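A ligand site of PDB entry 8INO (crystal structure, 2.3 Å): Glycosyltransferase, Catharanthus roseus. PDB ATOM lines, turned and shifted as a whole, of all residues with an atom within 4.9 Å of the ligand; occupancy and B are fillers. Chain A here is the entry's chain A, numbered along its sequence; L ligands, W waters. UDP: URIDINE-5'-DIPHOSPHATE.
Water W1 lies within hydrogen-bond range of O1B of the ligand (2.6 Å), N of Gly 14 (2.9 Å) and OG of Ser 286 (3.4 Å). Water W5 lies within hydrogen-bond range of O of Phe 284, O2B of the ligand, N of Leu 287, NE2 of His 357 and N of Ser 286. Water W2 lies within hydrogen-bond range of OE2 of Glu 365 (2.8 Å) and O3' of the ligand (2.9 Å). Water W3 lies within hydrogen-bond range of an oxygen (O2) of the ligand (3.0 Å), the indole nitrogen of Trp 339 (3.1 Å) and the side-chain amide nitrogen of Asn 17 (3.2 Å). Water W4 lies within hydrogen-bond range of the side-chain hydroxyl of Ser 283 (2.6 Å), the side-chain amide nitrogen of Gln 342 (2.7 Å) and the side-chain hydroxyl of Ser 362 (3.0 Å).
The backbone NH of Gln 342 lies close to the side-chain sulfur of Cys 340. N of Gly 285 is in hydrogen-bond range of OG of Ser 283 (3.2 Å). O of Lys 13 sits close to ND2 of Asn 17 (3.5 Å). The backbone carbonyl oxygen (O) of Gly 14 is in hydrogen-bond range of the side-chain amide nitrogen (ND2) of Asn 361 (2.6 Å). OH of Tyr 281 lies within hydrogen-bond range of SG of Cys 340, 3.1 Å away. NE2 of Gln 342 sits at hydrogen-bond distance from OH of Tyr 281. The side-chain amide oxygen (OE1) of Gln 342 lies close to the side-chain carboxylate (OE1) of Glu 365, at 2.9 Å. The side-chain amide oxygen of Gln 382 lies close to the backbone carbonyl oxygen of His 357.
A nitrogen (N3) of the ligand sits close to the indole nitrogen (NE1) of Trp 339 (3.4 Å). Residues that only touch the ligand: Gly 14 (3.5 Å), Tyr 281 (3.8 Å), Ser 283 (3.7 Å), Gly 285 (3.8 Å), Val 312 (3.2 Å) and Gly 359 (3.6 Å). Hydrophobic or aromatic side chains that line the ligand: Val 312, Trp 339 and His 357. 16 residues have an atom within 4 Å of the ligand: Gly 14, Asn 17, Tyr 281, Ser 283, Gly 285, Ser 286, Val 312, Trp 339, Cys 340, Gln 342, His 357, Gly 359, Trp 360, Asn 361, Ser 362 and Glu 365.
OE1 of Glu 365 sits at hydrogen-bond distance from O2' of the ligand, at 2.7 Å. O3B of the ligand sits at hydrogen-bond distance from OG of Ser 286 (2.6 Å). The side-chain amide oxygen (OE1) of Gln 342 lies within hydrogen-bond range of an oxygen (O2') of the ligand, 3.1 Å away. OG of Ser 362 sits at hydrogen-bond distance from O2A of the ligand (3.0 Å). ND2 of Asn 17 sits at hydrogen-bond distance from O3' of the ligand (3.0 Å). The backbone NH (N) of Ser 362 sits at hydrogen-bond distance from an oxygen (O2A) of the ligand, 2.9 Å away. ND2 of Asn 361 sits at hydrogen-bond distance from O1A of the ligand, 2.9 Å away. The backbone NH (N) of Asn 361 is in hydrogen-bond range of an oxygen (O1A) of the ligand, 3.1 Å away. O4 of the ligand is in hydrogen-bond range of SG of Cys 340, at 3.4 Å. O of Cys 340 is in hydrogen-bond range of N3 of the ligand (2.8 Å). A ring nitrogen (NE2) of His 357 lies within hydrogen-bond range of an oxygen (O3A) of the ligand (2.9 Å). The backbone NH of Trp 360 lies within hydrogen-bond range of an oxygen (O1A) of the ligand. O4 of the ligand sits at hydrogen-bond distance from N of Cys 340. O3B of the ligand sits at hydrogen-bond distance from N of Ser 286 (2.8 Å).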
ATOM      1  N   LYS A  13     -30.048 -23.450   5.561  1.00  0.00           N
ATOM      2  CA  LYS A  13     -28.834 -22.812   6.081  1.00  0.00           C
ATOM      3  C   LYS A  13     -29.091 -22.033   7.364  1.00  0.00           C
ATOM      4  O   LYS A  13     -28.243 -22.019   8.259  1.00  0.00           O
ATOM      5  CB  LYS A  13     -28.221 -21.909   5.016  1.00  0.00           C
ATOM      6  CG  LYS A  13     -27.625 -22.690   3.833  1.00  0.00           C
ATOM      7  CD  LYS A  13     -26.721 -21.788   2.989  1.00  0.00           C
ATOM      8  CE  LYS A  13     -26.337 -22.442   1.672  1.00  0.00           C
ATOM      9  NZ  LYS A  13     -27.310 -23.473   1.195  1.00  0.00           N
ATOM     10  N   GLY A  14     -30.262 -21.394   7.480  1.00  0.00           N
ATOM     11  CA  GLY A  14     -30.572 -20.683   8.718  1.00  0.00           C
ATOM     12  C   GLY A  14     -30.735 -21.581   9.930  1.00  0.00           C
ATOM     13  O   GLY A  14     -30.812 -21.079  11.050  1.00  0.00           O
ATOM     14  N   ASN A  17     -26.492 -23.468  10.139  1.00  0.00           N
ATOM     15  CA  ASN A  17     -25.367 -22.634  10.569  1.00  0.00           C
ATOM     16  C   ASN A  17     -25.303 -22.424  12.083  1.00  0.00           C
ATOM     17  O   ASN A  17     -24.238 -22.643  12.671  1.00  0.00           O
ATOM     18  CB  ASN A  17     -25.413 -21.291   9.825  1.00  0.00           C
ATOM     19  CG  ASN A  17     -25.060 -21.435   8.373  1.00  0.00           C
ATOM     20  OD1 ASN A  17     -24.609 -22.493   7.936  1.00  0.00           O
ATOM     21  ND2 ASN A  17     -25.263 -20.354   7.612  1.00  0.00           N
ATOM     22  N   TYR A 258     -17.682 -21.964   7.980  1.00  0.00           N
ATOM     23  CA  TYR A 258     -18.629 -22.102   6.890  1.00  0.00           C
ATOM     24  C   TYR A 258     -18.479 -23.454   6.217  1.00  0.00           C
ATOM     25  O   TYR A 258     -17.370 -23.928   5.979  1.00  0.00           O
ATOM     26  CB  TYR A 258     -18.438 -20.999   5.845  1.00  0.00           C
ATOM     27  CG  TYR A 258     -18.364 -19.587   6.373  1.00  0.00           C
ATOM     28  CD1 TYR A 258     -19.500 -18.912   6.792  1.00  0.00           C
ATOM     29  CD2 TYR A 258     -17.147 -18.908   6.408  1.00  0.00           C
ATOM     30  CE1 TYR A 258     -19.437 -17.593   7.256  1.00  0.00           C
ATOM     31  CE2 TYR A 258     -17.068 -17.608   6.868  1.00  0.00           C
ATOM     32  CZ  TYR A 258     -18.213 -16.950   7.292  1.00  0.00           C
ATOM     33  OH  TYR A 258     -18.136 -15.654   7.738  1.00  0.00           O
ATOM     34  N   TYR A 281     -24.459  -3.358   3.343  1.00  0.00           N
ATOM     35  CA  TYR A 281     -24.515  -4.789   3.096  1.00  0.00           C
ATOM     36  C   TYR A 281     -25.974  -5.184   2.912  1.00  0.00           C
ATOM     37  O   TYR A 281     -26.820  -4.864   3.748  1.00  0.00           O
ATOM     38  CB  TYR A 281     -23.871  -5.537   4.260  1.00  0.00           C
ATOM     39  CG  TYR A 281     -24.029  -7.033   4.177  1.00  0.00           C
ATOM     40  CD1 TYR A 281     -23.748  -7.737   2.999  1.00  0.00           C
ATOM     41  CD2 TYR A 281     -24.468  -7.755   5.284  1.00  0.00           C
ATOM     42  CE1 TYR A 281     -23.884  -9.116   2.929  1.00  0.00           C
ATOM     43  CE2 TYR A 281     -24.623  -9.142   5.233  1.00  0.00           C
ATOM     44  CZ  TYR A 281     -24.341  -9.810   4.060  1.00  0.00           C
ATOM     45  OH  TYR A 281     -24.487 -11.192   4.043  1.00  0.00           O
ATOM     46  N   SER A 283     -28.704  -8.285   2.035  1.00  0.00           N
ATOM     47  CA  SER A 283     -28.912  -9.721   1.884  1.00  0.00           C
ATOM     48  C   SER A 283     -30.303 -10.084   2.358  1.00  0.00           C
ATOM     49  O   SER A 283     -30.747  -9.606   3.402  1.00  0.00           O
ATOM     50  CB  SER A 283     -27.866 -10.538   2.655  1.00  0.00           C
ATOM     51  OG  SER A 283     -28.197 -11.918   2.625  1.00  0.00           O
ATOM     52  N   PHE A 284     -30.966 -10.969   1.619  1.00  0.00           N
ATOM     53  CA  PHE A 284     -32.263 -11.485   2.027  1.00  0.00           C
ATOM     54  C   PHE A 284     -32.181 -12.950   2.440  1.00  0.00           C
ATOM     55  O   PHE A 284     -33.200 -13.652   2.487  1.00  0.00           O
ATOM     56  CB  PHE A 284     -33.264 -11.232   0.906  1.00  0.00           C
ATOM     57  CG  PHE A 284     -33.583  -9.766   0.750  1.00  0.00           C
ATOM     58  CD1 PHE A 284     -32.718  -8.931   0.050  1.00  0.00           C
ATOM     59  CD2 PHE A 284     -34.687  -9.219   1.372  1.00  0.00           C
ATOM     60  CE1 PHE A 284     -32.977  -7.589  -0.046  1.00  0.00           C
ATOM     61  CE2 PHE A 284     -34.953  -7.876   1.269  1.00  0.00           C
ATOM     62  CZ  PHE A 284     -34.098  -7.061   0.560  1.00  0.00           C
ATOM     63  N   GLY A 285     -30.987 -13.421   2.792  1.00  0.00           N
ATOM     64  CA  GLY A 285     -30.838 -14.731   3.380  1.00  0.00           C
ATOM     65  C   GLY A 285     -30.747 -15.831   2.337  1.00  0.00           C
ATOM     66  O   GLY A 285     -30.423 -15.620   1.167  1.00  0.00           O
ATOM     67  N   SER A 286     -31.043 -17.050   2.806  1.00  0.00           N
ATOM     68  CA  SER A 286     -30.902 -18.271   2.021  1.00  0.00           C
ATOM     69  C   SER A 286     -32.196 -18.746   1.382  1.00  0.00           C
ATOM     70  O   SER A 286     -32.137 -19.604   0.503  1.00  0.00           O
ATOM     71  CB  SER A 286     -30.358 -19.402   2.916  1.00  0.00           C
ATOM     72  OG  SER A 286     -31.322 -19.781   3.902  1.00  0.00           O
ATOM     73  N   LEU A 287     -33.359 -18.215   1.772  1.00  0.00           N
ATOM     74  CA  LEU A 287     -34.594 -18.699   1.158  1.00  0.00           C
ATOM     75  C   LEU A 287     -35.423 -17.640   0.469  1.00  0.00           C
ATOM     76  O   LEU A 287     -35.924 -17.892  -0.621  1.00  0.00           O
ATOM     77  CB  LEU A 287     -35.481 -19.419   2.190  1.00  0.00           C
ATOM     78  CG  LEU A 287     -34.820 -20.501   3.004  1.00  0.00           C
ATOM     79  CD1 LEU A 287     -35.414 -20.631   4.421  1.00  0.00           C
ATOM     80  CD2 LEU A 287     -34.948 -21.802   2.220  1.00  0.00           C
ATOM     81  N   VAL A 312     -25.757  -9.619  -1.690  1.00  0.00           N
ATOM     82  CA  VAL A 312     -25.857 -11.061  -1.923  1.00  0.00           C
ATOM     83  C   VAL A 312     -27.148 -11.346  -2.689  1.00  0.00           C
ATOM     84  O   VAL A 312     -28.244 -11.280  -2.149  1.00  0.00           O
ATOM     85  CB  VAL A 312     -25.825 -11.851  -0.617  1.00  0.00           C
ATOM     86  CG1 VAL A 312     -25.897 -13.339  -0.930  1.00  0.00           C
ATOM     87  CG2 VAL A 312     -24.568 -11.554   0.171  1.00  0.00           C
ATOM     88  N   TRP A 339     -22.985 -15.333  -2.680  1.00  0.00           N
ATOM     89  CA  TRP A 339     -22.910 -15.716  -1.272  1.00  0.00           C
ATOM     90  C   TRP A 339     -21.627 -15.114  -0.728  1.00  0.00           C
ATOM     91  O   TRP A 339     -20.660 -14.943  -1.481  1.00  0.00           O
ATOM     92  CB  TRP A 339     -22.926 -17.251  -1.103  1.00  0.00           C
ATOM     93  CG  TRP A 339     -23.435 -17.744   0.218  1.00  0.00           C
ATOM     94  CD1 TRP A 339     -22.735 -18.447   1.148  1.00  0.00           C
ATOM     95  CD2 TRP A 339     -24.771 -17.607   0.742  1.00  0.00           C
ATOM     96  NE1 TRP A 339     -23.546 -18.742   2.238  1.00  0.00           N
ATOM     97  CE2 TRP A 339     -24.796 -18.234   2.007  1.00  0.00           C
ATOM     98  CE3 TRP A 339     -25.930 -16.995   0.265  1.00  0.00           C
ATOM     99  CZ2 TRP A 339     -25.940 -18.282   2.791  1.00  0.00           C
ATOM    100  CZ3 TRP A 339     -27.084 -17.046   1.058  1.00  0.00           C
ATOM    101  CH2 TRP A 339     -27.068 -17.686   2.307  1.00  0.00           C
ATOM    102  N   CYS A 340     -21.618 -14.777   0.549  1.00  0.00           N
ATOM    103  CA  CYS A 340     -20.496 -14.064   1.147  1.00  0.00           C
ATOM    104  C   CYS A 340     -20.219 -14.638   2.531  1.00  0.00           C
ATOM    105  O   CYS A 340     -21.039 -15.364   3.091  1.00  0.00           O
ATOM    106  CB  CYS A 340     -20.794 -12.562   1.235  1.00  0.00           C
ATOM    107  SG  CYS A 340     -21.787 -12.048   2.673  1.00  0.00           S
ATOM    108  N   GLN A 342     -20.768 -13.994   5.700  1.00  0.00           N
ATOM    109  CA  GLN A 342     -21.586 -12.968   6.347  1.00  0.00           C
ATOM    110  C   GLN A 342     -20.996 -12.547   7.694  1.00  0.00           C
ATOM    111  O   GLN A 342     -20.998 -11.360   8.028  1.00  0.00           O
ATOM    112  CB  GLN A 342     -23.042 -13.448   6.506  1.00  0.00           C
ATOM    113  CG  GLN A 342     -23.895 -12.525   7.415  1.00  0.00           C
ATOM    114  CD  GLN A 342     -25.405 -12.575   7.160  1.00  0.00           C
ATOM    115  OE1 GLN A 342     -26.192 -12.721   8.095  1.00  0.00           O
ATOM    116  NE2 GLN A 342     -25.812 -12.386   5.896  1.00  0.00           N
ATOM    117  N   LEU A 343     -20.485 -13.496   8.497  1.00  0.00           N
ATOM    118  CA  LEU A 343     -19.859 -13.136   9.768  1.00  0.00           C
ATOM    119  C   LEU A 343     -18.652 -12.212   9.569  1.00  0.00           C
ATOM    120  O   LEU A 343     -18.475 -11.232  10.302  1.00  0.00           O
ATOM    121  CB  LEU A 343     -19.429 -14.386  10.541  1.00  0.00           C
ATOM    122  CG  LEU A 343     -20.484 -15.483  10.855  1.00  0.00           C
ATOM    123  CD1 LEU A 343     -19.909 -16.652  11.668  1.00  0.00           C
ATOM    124  CD2 LEU A 343     -21.726 -14.928  11.561  1.00  0.00           C
ATOM    125  N   HIS A 357     -33.553  -9.078   5.483  1.00  0.00           N
ATOM    126  CA  HIS A 357     -34.887  -9.668   5.612  1.00  0.00           C
ATOM    127  C   HIS A 357     -35.254 -10.031   7.057  1.00  0.00           C
ATOM    128  O   HIS A 357     -36.378 -10.480   7.301  1.00  0.00           O
ATOM    129  CB  HIS A 357     -35.007 -10.918   4.743  1.00  0.00           C
ATOM    130  CG  HIS A 357     -34.342 -12.136   5.325  1.00  0.00           C
ATOM    131  ND1 HIS A 357     -33.064 -12.109   5.841  1.00  0.00           N
ATOM    132  CD2 HIS A 357     -34.769 -13.415   5.456  1.00  0.00           C
ATOM    133  CE1 HIS A 357     -32.742 -13.317   6.271  1.00  0.00           C
ATOM    134  NE2 HIS A 357     -33.759 -14.129   6.052  1.00  0.00           N
ATOM    135  N   GLY A 359     -34.244 -12.421   9.147  1.00  0.00           N
ATOM    136  CA  GLY A 359     -34.070 -13.730   9.740  1.00  0.00           C
ATOM    137  C   GLY A 359     -33.279 -13.636  11.023  1.00  0.00           C
ATOM    138  O   GLY A 359     -32.497 -12.712  11.215  1.00  0.00           O
ATOM    139  N   TRP A 360     -33.499 -14.585  11.924  1.00  0.00           N
ATOM    140  CA  TRP A 360     -32.950 -14.408  13.268  1.00  0.00           C
ATOM    141  C   TRP A 360     -31.419 -14.458  13.282  1.00  0.00           C
ATOM    142  O   TRP A 360     -30.790 -13.696  14.018  1.00  0.00           O
ATOM    143  CB  TRP A 360     -33.529 -15.443  14.246  1.00  0.00           C
ATOM    144  CG  TRP A 360     -32.916 -15.263  15.584  1.00  0.00           C
ATOM    145  CD1 TRP A 360     -32.190 -16.187  16.301  1.00  0.00           C
ATOM    146  CD2 TRP A 360     -32.915 -14.071  16.376  1.00  0.00           C
ATOM    147  NE1 TRP A 360     -31.755 -15.652  17.482  1.00  0.00           N
ATOM    148  CE2 TRP A 360     -32.187 -14.342  17.557  1.00  0.00           C
ATOM    149  CE3 TRP A 360     -33.464 -12.789  16.205  1.00  0.00           C
ATOM    150  CZ2 TRP A 360     -32.004 -13.392  18.551  1.00  0.00           C
ATOM    151  CZ3 TRP A 360     -33.275 -11.860  17.176  1.00  0.00           C
ATOM    152  CH2 TRP A 360     -32.550 -12.156  18.340  1.00  0.00           C
ATOM    153  N   ASN A 361     -30.801 -15.363  12.500  1.00  0.00           N
ATOM    154  CA  ASN A 361     -29.334 -15.401  12.452  1.00  0.00           C
ATOM    155  C   ASN A 361     -28.754 -14.072  11.988  1.00  0.00           C
ATOM    156  O   ASN A 361     -27.795 -13.549  12.574  1.00  0.00           O
ATOM    157  CB  ASN A 361     -28.837 -16.527  11.538  1.00  0.00           C
ATOM    158  CG  ASN A 361     -29.141 -17.913  12.084  1.00  0.00           C
ATOM    159  OD1 ASN A 361     -28.546 -18.348  13.069  1.00  0.00           O
ATOM    160  ND2 ASN A 361     -30.073 -18.601  11.440  1.00  0.00           N
ATOM    161  N   SER A 362     -29.317 -13.520  10.906  1.00  0.00           N
ATOM    162  CA  SER A 362     -28.826 -12.251  10.407  1.00  0.00           C
ATOM    163  C   SER A 362     -29.049 -11.134  11.414  1.00  0.00           C
ATOM    164  O   SER A 362     -28.174 -10.278  11.599  1.00  0.00           O
ATOM    165  CB  SER A 362     -29.501 -11.934   9.079  1.00  0.00           C
ATOM    166  OG  SER A 362     -28.848 -12.652   8.051  1.00  0.00           O
ATOM    167  N   GLU A 365     -26.594 -11.716  14.319  1.00  0.00           N
ATOM    168  CA  GLU A 365     -25.198 -11.480  13.845  1.00  0.00           C
ATOM    169  C   GLU A 365     -24.888  -9.980  13.745  1.00  0.00           C
ATOM    170  O   GLU A 365     -23.826  -9.593  14.216  1.00  0.00           O
ATOM    171  CB  GLU A 365     -24.909 -12.239  12.562  1.00  0.00           C
ATOM    172  CG  GLU A 365     -24.708 -13.721  12.792  1.00  0.00           C
ATOM    173  CD  GLU A 365     -25.102 -14.594  11.609  1.00  0.00           C
ATOM    174  OE1 GLU A 365     -25.156 -14.069  10.493  1.00  0.00           O
ATOM    175  OE2 GLU A 365     -25.348 -15.779  11.802  1.00  0.00           O
ATOM    176  N   GLN A 382     -39.736 -13.114  10.476  1.00  0.00           N
ATOM    177  CA  GLN A 382     -39.019 -11.908  10.080  1.00  0.00           C
ATOM    178  C   GLN A 382     -39.797 -10.649  10.455  1.00  0.00           C
ATOM    179  O   GLN A 382     -39.206  -9.642  10.872  1.00  0.00           O
ATOM    180  CB  GLN A 382     -38.738 -11.955   8.575  1.00  0.00           C
ATOM    181  CG  GLN A 382     -37.844 -13.114   8.142  1.00  0.00           C
ATOM    182  CD  GLN A 382     -38.082 -13.518   6.699  1.00  0.00           C
ATOM    183  OE1 GLN A 382     -38.461 -12.688   5.855  1.00  0.00           O
ATOM    184  NE2 GLN A 382     -37.878 -14.788   6.403  1.00  0.00           N
HETATM  185  N1  UDP L   1     -25.398 -16.116   5.196  1.00  0.00           N
HETATM  186  C2  UDP L   1     -24.180 -16.222   4.713  1.00  0.00           C
HETATM  187  N3  UDP L   1     -23.786 -15.614   3.615  1.00  0.00           N
HETATM  188  C4  UDP L   1     -24.654 -14.879   2.964  1.00  0.00           C
HETATM  189  C5  UDP L   1     -25.973 -14.724   3.416  1.00  0.00           C
HETATM  190  C6  UDP L   1     -26.331 -15.387   4.582  1.00  0.00           C
HETATM  191  O2  UDP L   1     -23.219 -16.989   5.363  1.00  0.00           O
HETATM  192  O4  UDP L   1     -24.214 -14.274   1.804  1.00  0.00           O
HETATM  193  C1' UDP L   1     -25.758 -16.832   6.412  1.00  0.00           C
HETATM  194  C2' UDP L   1     -26.133 -15.925   7.594  1.00  0.00           C
HETATM  195  O2' UDP L   1     -24.992 -15.578   8.293  1.00  0.00           O
HETATM  196  C3' UDP L   1     -27.036 -16.929   8.360  1.00  0.00           C
HETATM  197  C4' UDP L   1     -27.738 -17.565   7.433  1.00  0.00           C
HETATM  198  O4' UDP L   1     -26.863 -17.480   6.110  1.00  0.00           O
HETATM  199  O3' UDP L   1     -26.120 -17.900   9.020  1.00  0.00           O
HETATM  200  C5' UDP L   1     -29.086 -16.937   7.109  1.00  0.00           C
HETATM  201  O5' UDP L   1     -29.872 -17.174   8.241  1.00  0.00           O
HETATM  202  PA  UDP L   1     -31.180 -16.262   8.619  1.00  0.00           P
HETATM  203  O1A UDP L   1     -31.768 -16.741   9.937  1.00  0.00           O
HETATM  204  O2A UDP L   1     -30.749 -14.813   8.732  1.00  0.00           O
HETATM  205  O3A UDP L   1     -32.336 -16.250   7.439  1.00  0.00           O
HETATM  206  PB  UDP L   1     -32.814 -17.487   6.476  1.00  0.00           P
HETATM  207  O1B UDP L   1     -33.072 -18.710   7.351  1.00  0.00           O
HETATM  208  O2B UDP L   1     -34.088 -17.032   5.785  1.00  0.00           O
HETATM  209  O3B UDP L   1     -31.741 -17.778   5.430  1.00  0.00           O
HETATM  210  O   HOH W   1     -32.960 -21.210   6.536  1.00  0.00           O
HETATM  211  O   HOH W   2     -23.704 -17.772  10.683  1.00  0.00           O
HETATM  212  O   HOH W   3     -23.309 -19.951   5.072  1.00  0.00           O
HETATM  213  O   HOH W   4     -28.386 -12.830   5.099  1.00  0.00           O
HETATM  214  O   HOH W   5     -34.138 -15.927   3.360  1.00  0.00           O
